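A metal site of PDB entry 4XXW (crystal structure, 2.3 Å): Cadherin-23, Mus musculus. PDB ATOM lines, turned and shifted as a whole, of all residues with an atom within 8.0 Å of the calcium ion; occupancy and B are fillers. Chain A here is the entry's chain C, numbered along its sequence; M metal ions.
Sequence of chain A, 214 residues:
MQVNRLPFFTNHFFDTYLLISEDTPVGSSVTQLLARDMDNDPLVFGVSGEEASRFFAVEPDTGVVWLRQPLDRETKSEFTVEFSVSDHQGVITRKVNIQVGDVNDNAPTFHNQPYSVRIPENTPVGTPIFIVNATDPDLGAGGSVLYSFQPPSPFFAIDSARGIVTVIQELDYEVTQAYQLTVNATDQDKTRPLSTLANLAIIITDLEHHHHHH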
ATOM      1  N   VAL A   3     -27.143  -4.874  33.064  1.00  0.00           N
ATOM      2  CA  VAL A   3     -26.334  -3.832  32.413  1.00  0.00           C
ATOM      3  C   VAL A   3     -26.062  -4.460  31.046  1.00  0.00           C
ATOM      4  O   VAL A   3     -26.165  -5.694  30.864  1.00  0.00           O
ATOM      5  CB  VAL A   3     -25.026  -3.421  33.213  1.00  0.00           C
ATOM      6  CG1 VAL A   3     -23.999  -2.672  32.359  1.00  0.00           C
ATOM      7  CG2 VAL A   3     -25.349  -2.511  34.393  1.00  0.00           C
ATOM      8  N   ASN A   4     -25.817  -3.611  30.072  1.00  0.00           N
ATOM      9  CA  ASN A   4     -25.435  -4.035  28.741  1.00  0.00           C
ATOM     10  C   ASN A   4     -24.185  -4.920  28.798  1.00  0.00           C
ATOM     11  O   ASN A   4     -23.210  -4.552  29.487  1.00  0.00           O
ATOM     12  CB  ASN A   4     -25.161  -2.827  27.860  1.00  0.00           C
ATOM     13  CG  ASN A   4     -24.710  -3.227  26.450  1.00  0.00           C
ATOM     14  OD1 ASN A   4     -25.299  -4.125  25.827  1.00  0.00           O
ATOM     15  ND2 ASN A   4     -23.664  -2.576  25.937  1.00  0.00           N
ATOM     16  N   ARG A   5     -24.215  -6.095  28.183  1.00  0.00           N
ATOM     17  CA  ARG A   5     -22.963  -6.819  27.815  1.00  0.00           C
ATOM     18  C   ARG A   5     -22.351  -6.233  26.478  1.00  0.00           C
ATOM     19  O   ARG A   5     -23.026  -6.162  25.431  1.00  0.00           O
ATOM     20  CB  ARG A   5     -23.180  -8.313  27.652  1.00  0.00           C
ATOM     21  CG  ARG A   5     -23.206  -9.227  28.904  1.00  0.00           C
ATOM     22  CD  ARG A   5     -24.462  -9.271  29.672  1.00  0.00           C
ATOM     23  NE  ARG A   5     -25.665  -9.549  28.893  1.00  0.00           N
ATOM     24  CZ  ARG A   5     -26.439 -10.664  29.007  1.00  0.00           C
ATOM     25  NH1 ARG A   5     -26.085 -11.642  29.769  1.00  0.00           N
ATOM     26  NH2 ARG A   5     -27.558 -10.803  28.277  1.00  0.00           N
ATOM     27  N   LEU A   6     -21.097  -5.840  26.503  1.00  0.00           N
ATOM     28  CA  LEU A   6     -20.450  -5.356  25.271  1.00  0.00           C
ATOM     29  C   LEU A   6     -20.092  -6.506  24.319  1.00  0.00           C
ATOM     30  O   LEU A   6     -19.776  -7.620  24.753  1.00  0.00           O
ATOM     31  CB  LEU A   6     -19.236  -4.518  25.586  1.00  0.00           C
ATOM     32  CG  LEU A   6     -19.514  -3.218  26.370  1.00  0.00           C
ATOM     33  CD1 LEU A   6     -18.247  -2.846  27.148  1.00  0.00           C
ATOM     34  CD2 LEU A   6     -19.983  -2.071  25.437  1.00  0.00           C
ATOM     35  N   PRO A   7     -20.170  -6.265  23.014  1.00  0.00           N
ATOM     36  CA  PRO A   7     -19.676  -7.293  22.064  1.00  0.00           C
ATOM     37  C   PRO A   7     -18.194  -7.395  22.005  1.00  0.00           C
ATOM     38  O   PRO A   7     -17.437  -6.466  22.425  1.00  0.00           O
ATOM     39  CB  PRO A   7     -20.161  -6.802  20.706  1.00  0.00           C
ATOM     40  CG  PRO A   7     -20.164  -5.313  20.851  1.00  0.00           C
ATOM     41  CD  PRO A   7     -20.486  -4.999  22.320  1.00  0.00           C
ATOM     42  N   ARG A  36     -19.445 -11.362  18.841  1.00  0.00           N
ATOM     43  CA  ARG A  36     -20.594 -11.900  19.586  1.00  0.00           C
ATOM     44  C   ARG A  36     -21.041 -10.884  20.651  1.00  0.00           C
ATOM     45  O   ARG A  36     -20.218 -10.284  21.299  1.00  0.00           O
ATOM     46  CB  ARG A  36     -20.127 -13.198  20.215  1.00  0.00           C
ATOM     47  CG  ARG A  36     -20.954 -13.779  21.337  1.00  0.00           C
ATOM     48  CD  ARG A  36     -22.254 -14.263  20.799  1.00  0.00           C
ATOM     49  NE  ARG A  36     -23.007 -14.980  21.828  1.00  0.00           N
ATOM     50  CZ  ARG A  36     -24.319 -14.948  21.964  1.00  0.00           C
ATOM     51  NH1 ARG A  36     -25.058 -14.223  21.128  1.00  0.00           N
ATOM     52  NH2 ARG A  36     -24.904 -15.643  22.945  1.00  0.00           N
ATOM     53  N   ASP A  37     -22.337 -10.727  20.861  1.00  0.00           N
ATOM     54  CA  ASP A  37     -22.889  -9.918  21.943  1.00  0.00           C
ATOM     55  C   ASP A  37     -23.820 -10.813  22.665  1.00  0.00           C
ATOM     56  O   ASP A  37     -24.761 -11.282  22.081  1.00  0.00           O
ATOM     57  CB  ASP A  37     -23.699  -8.769  21.279  1.00  0.00           C
ATOM     58  CG  ASP A  37     -24.240  -7.748  22.282  1.00  0.00           C
ATOM     59  OD1 ASP A  37     -25.178  -8.046  23.064  1.00  0.00           O
ATOM     60  OD2 ASP A  37     -23.720  -6.617  22.258  1.00  0.00           O
ATOM     61  N   MET A  38     -23.643 -11.044  23.957  1.00  0.00           N
ATOM     62  CA  MET A  38     -24.500 -11.974  24.665  1.00  0.00           C
ATOM     63  C   MET A  38     -25.947 -11.476  24.840  1.00  0.00           C
ATOM     64  O   MET A  38     -26.806 -12.249  25.144  1.00  0.00           O
ATOM     65  CB  MET A  38     -23.871 -12.294  26.004  1.00  0.00           C
ATOM     66  CG  MET A  38     -22.523 -13.051  25.838  1.00  0.00           C
ATOM     67  SD  MET A  38     -21.476 -13.007  27.307  1.00  0.00           S
ATOM     68  CE  MET A  38     -22.613 -13.362  28.616  1.00  0.00           C
ATOM     69  N   ASP A  39     -26.201 -10.182  24.631  1.00  0.00           N
ATOM     70  CA  ASP A  39     -27.575  -9.693  24.540  1.00  0.00           C
ATOM     71  C   ASP A  39     -28.220 -10.067  23.174  1.00  0.00           C
ATOM     72  O   ASP A  39     -29.418  -9.953  23.033  1.00  0.00           O
ATOM     73  CB  ASP A  39     -27.682  -8.133  24.731  1.00  0.00           C
ATOM     74  CG  ASP A  39     -26.887  -7.645  25.948  1.00  0.00           C
ATOM     75  OD1 ASP A  39     -27.225  -8.148  27.008  1.00  0.00           O
ATOM     76  OD2 ASP A  39     -25.918  -6.829  25.798  1.00  0.00           O
ATOM     77  N   ASN A  40     -27.393 -10.421  22.202  1.00  0.00           N
ATOM     78  CA  ASN A  40     -27.725 -10.568  20.823  1.00  0.00           C
ATOM     79  C   ASN A  40     -28.189  -9.220  20.213  1.00  0.00           C
ATOM     80  O   ASN A  40     -29.020  -9.180  19.349  1.00  0.00           O
ATOM     81  CB  ASN A  40     -28.752 -11.670  20.608  1.00  0.00           C
ATOM     82  CG  ASN A  40     -28.717 -12.216  19.203  1.00  0.00           C
ATOM     83  OD1 ASN A  40     -27.707 -12.079  18.519  1.00  0.00           O
ATOM     84  ND2 ASN A  40     -29.823 -12.829  18.755  1.00  0.00           N
ATOM     85  N   ASP A  41     -27.647  -8.121  20.720  1.00  0.00           N
ATOM     86  CA  ASP A  41     -27.932  -6.778  20.131  1.00  0.00           C
ATOM     87  C   ASP A  41     -27.518  -6.804  18.657  1.00  0.00           C
ATOM     88  O   ASP A  41     -26.541  -7.473  18.340  1.00  0.00           O
ATOM     89  CB  ASP A  41     -27.148  -5.657  20.835  1.00  0.00           C
ATOM     90  CG  ASP A  41     -27.643  -5.396  22.246  1.00  0.00           C
ATOM     91  OD1 ASP A  41     -28.883  -5.451  22.442  1.00  0.00           O
ATOM     92  OD2 ASP A  41     -26.813  -5.195  23.179  1.00  0.00           O
ATOM     93  N   PRO A  42     -28.286  -6.122  17.770  1.00  0.00           N
ATOM     94  CA  PRO A  42     -27.809  -5.800  16.433  1.00  0.00           C
ATOM     95  C   PRO A  42     -26.442  -5.128  16.517  1.00  0.00           C
ATOM     96  O   PRO A  42     -26.192  -4.328  17.390  1.00  0.00           O
ATOM     97  CB  PRO A  42     -28.886  -4.843  15.845  1.00  0.00           C
ATOM     98  CG  PRO A  42     -30.071  -4.954  16.760  1.00  0.00           C
ATOM     99  CD  PRO A  42     -29.539  -5.409  18.090  1.00  0.00           C
ATOM    100  N   LEU A  43     -25.528  -5.604  15.696  1.00  0.00           N
ATOM    101  CA  LEU A  43     -24.184  -5.113  15.708  1.00  0.00           C
ATOM    102  C   LEU A  43     -23.885  -4.291  14.443  1.00  0.00           C
ATOM    103  O   LEU A  43     -24.381  -4.603  13.369  1.00  0.00           O
ATOM    104  CB  LEU A  43     -23.239  -6.312  15.880  1.00  0.00           C
ATOM    105  CG  LEU A  43     -23.409  -6.979  17.273  1.00  0.00           C
ATOM    106  CD1 LEU A  43     -22.306  -8.008  17.405  1.00  0.00           C
ATOM    107  CD2 LEU A  43     -23.349  -6.020  18.460  1.00  0.00           C
ATOM    108  N   SER A  86     -20.116  -2.287  17.234  1.00  0.00           N
ATOM    109  CA  SER A  86     -20.906  -1.487  18.135  1.00  0.00           C
ATOM    110  C   SER A  86     -22.275  -2.102  18.345  1.00  0.00           C
ATOM    111  O   SER A  86     -22.864  -2.554  17.396  1.00  0.00           O
ATOM    112  CB  SER A  86     -21.016  -0.049  17.585  1.00  0.00           C
ATOM    113  OG  SER A  86     -21.589   0.691  18.621  1.00  0.00           O
ATOM    114  N   ASP A  87     -22.748  -2.105  19.590  1.00  0.00           N
ATOM    115  CA  ASP A  87     -24.150  -2.394  19.850  1.00  0.00           C
ATOM    116  C   ASP A  87     -25.014  -1.152  20.067  1.00  0.00           C
ATOM    117  O   ASP A  87     -26.133  -1.257  20.561  1.00  0.00           O
ATOM    118  CB  ASP A  87     -24.297  -3.406  20.982  1.00  0.00           C
ATOM    119  CG  ASP A  87     -23.797  -2.905  22.321  1.00  0.00           C
ATOM    120  OD1 ASP A  87     -23.396  -1.717  22.398  1.00  0.00           O
ATOM    121  OD2 ASP A  87     -23.773  -3.667  23.283  1.00  0.00           O
ATOM    122  N   HIS A  88     -24.503   0.031  19.683  1.00  0.00           N
ATOM    123  CA  HIS A  88     -25.224   1.340  19.884  1.00  0.00           C
ATOM    124  C   HIS A  88     -25.353   1.737  21.385  1.00  0.00           C
ATOM    125  O   HIS A  88     -26.289   2.433  21.767  1.00  0.00           O
ATOM    126  CB  HIS A  88     -26.643   1.377  19.209  1.00  0.00           C
ATOM    127  CG  HIS A  88     -26.633   1.078  17.729  1.00  0.00           C
ATOM    128  ND1 HIS A  88     -26.449   2.046  16.760  1.00  0.00           N
ATOM    129  CD2 HIS A  88     -26.771  -0.097  17.052  1.00  0.00           C
ATOM    130  CE1 HIS A  88     -26.500   1.493  15.563  1.00  0.00           C
ATOM    131  NE2 HIS A  88     -26.689   0.195  15.704  1.00  0.00           N
ATOM    132  N   GLN A  89     -24.451   1.198  22.208  1.00  0.00           N
ATOM    133  CA  GLN A  89     -24.252   1.623  23.586  1.00  0.00           C
ATOM    134  C   GLN A  89     -22.773   1.664  23.936  1.00  0.00           C
ATOM    135  O   GLN A  89     -22.364   1.955  25.056  1.00  0.00           O
ATOM    136  CB  GLN A  89     -24.957   0.609  24.467  1.00  0.00           C
ATOM    137  CG  GLN A  89     -26.424   0.462  24.101  1.00  0.00           C
ATOM    138  CD  GLN A  89     -27.129  -0.638  24.867  1.00  0.00           C
ATOM    139  OE1 GLN A  89     -27.296  -0.532  26.085  1.00  0.00           O
ATOM    140  NE2 GLN A  89     -27.518  -1.735  24.144  1.00  0.00           N
ATOM    141  N   GLY A  90     -21.942   1.378  22.959  1.00  0.00           N
ATOM    142  CA  GLY A  90     -20.544   1.084  23.189  1.00  0.00           C
ATOM    143  C   GLY A  90     -19.922   0.780  21.859  1.00  0.00           C
ATOM    144  O   GLY A  90     -20.496   0.036  21.068  1.00  0.00           O
HETATM  145 CA    CA M   1     -24.852  -5.603  24.139  1.00  0.00          CA
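The side-chain carboxylate of Asp 87 lies within hydrogen-bond range of the backbone NH of Gln 89 (3.1 Å).
The backbone NH of Gly 90 sits at hydrogen-bond distance from the side-chain carboxylate of Asp 87 (3.5 Å).
N of Asn 40 sits close to OD1 of Asp 37 (3.4 Å).
Of the 18 residues printed, 6 come within 4 Å of the calcium ion.
The nearest printed residue that does not touch the calcium ion is Leu 6 (4.4 Å).
The calcium ion is bound by OD2 of Asp 41 (2.2 Å).
The calcium ion is bound by the side-chain amide oxygen (OD1) of Asn 4 (2.3 Å).
O of Arg 5 is bound to the calcium ion (2.3 Å).
The calcium ion is bound by OD2 of Asp 39 (2.3 Å).
The calcium ion is bound by OD2 of Asp 87, at 2.4 Å.
The calcium ion is bound by the side-chain carboxylate (OD2) of Asp 37 (2.4 Å).
The side-chain carboxylate (OD1) of Asp 37 is bound to the calcium ion (2.7 Å).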
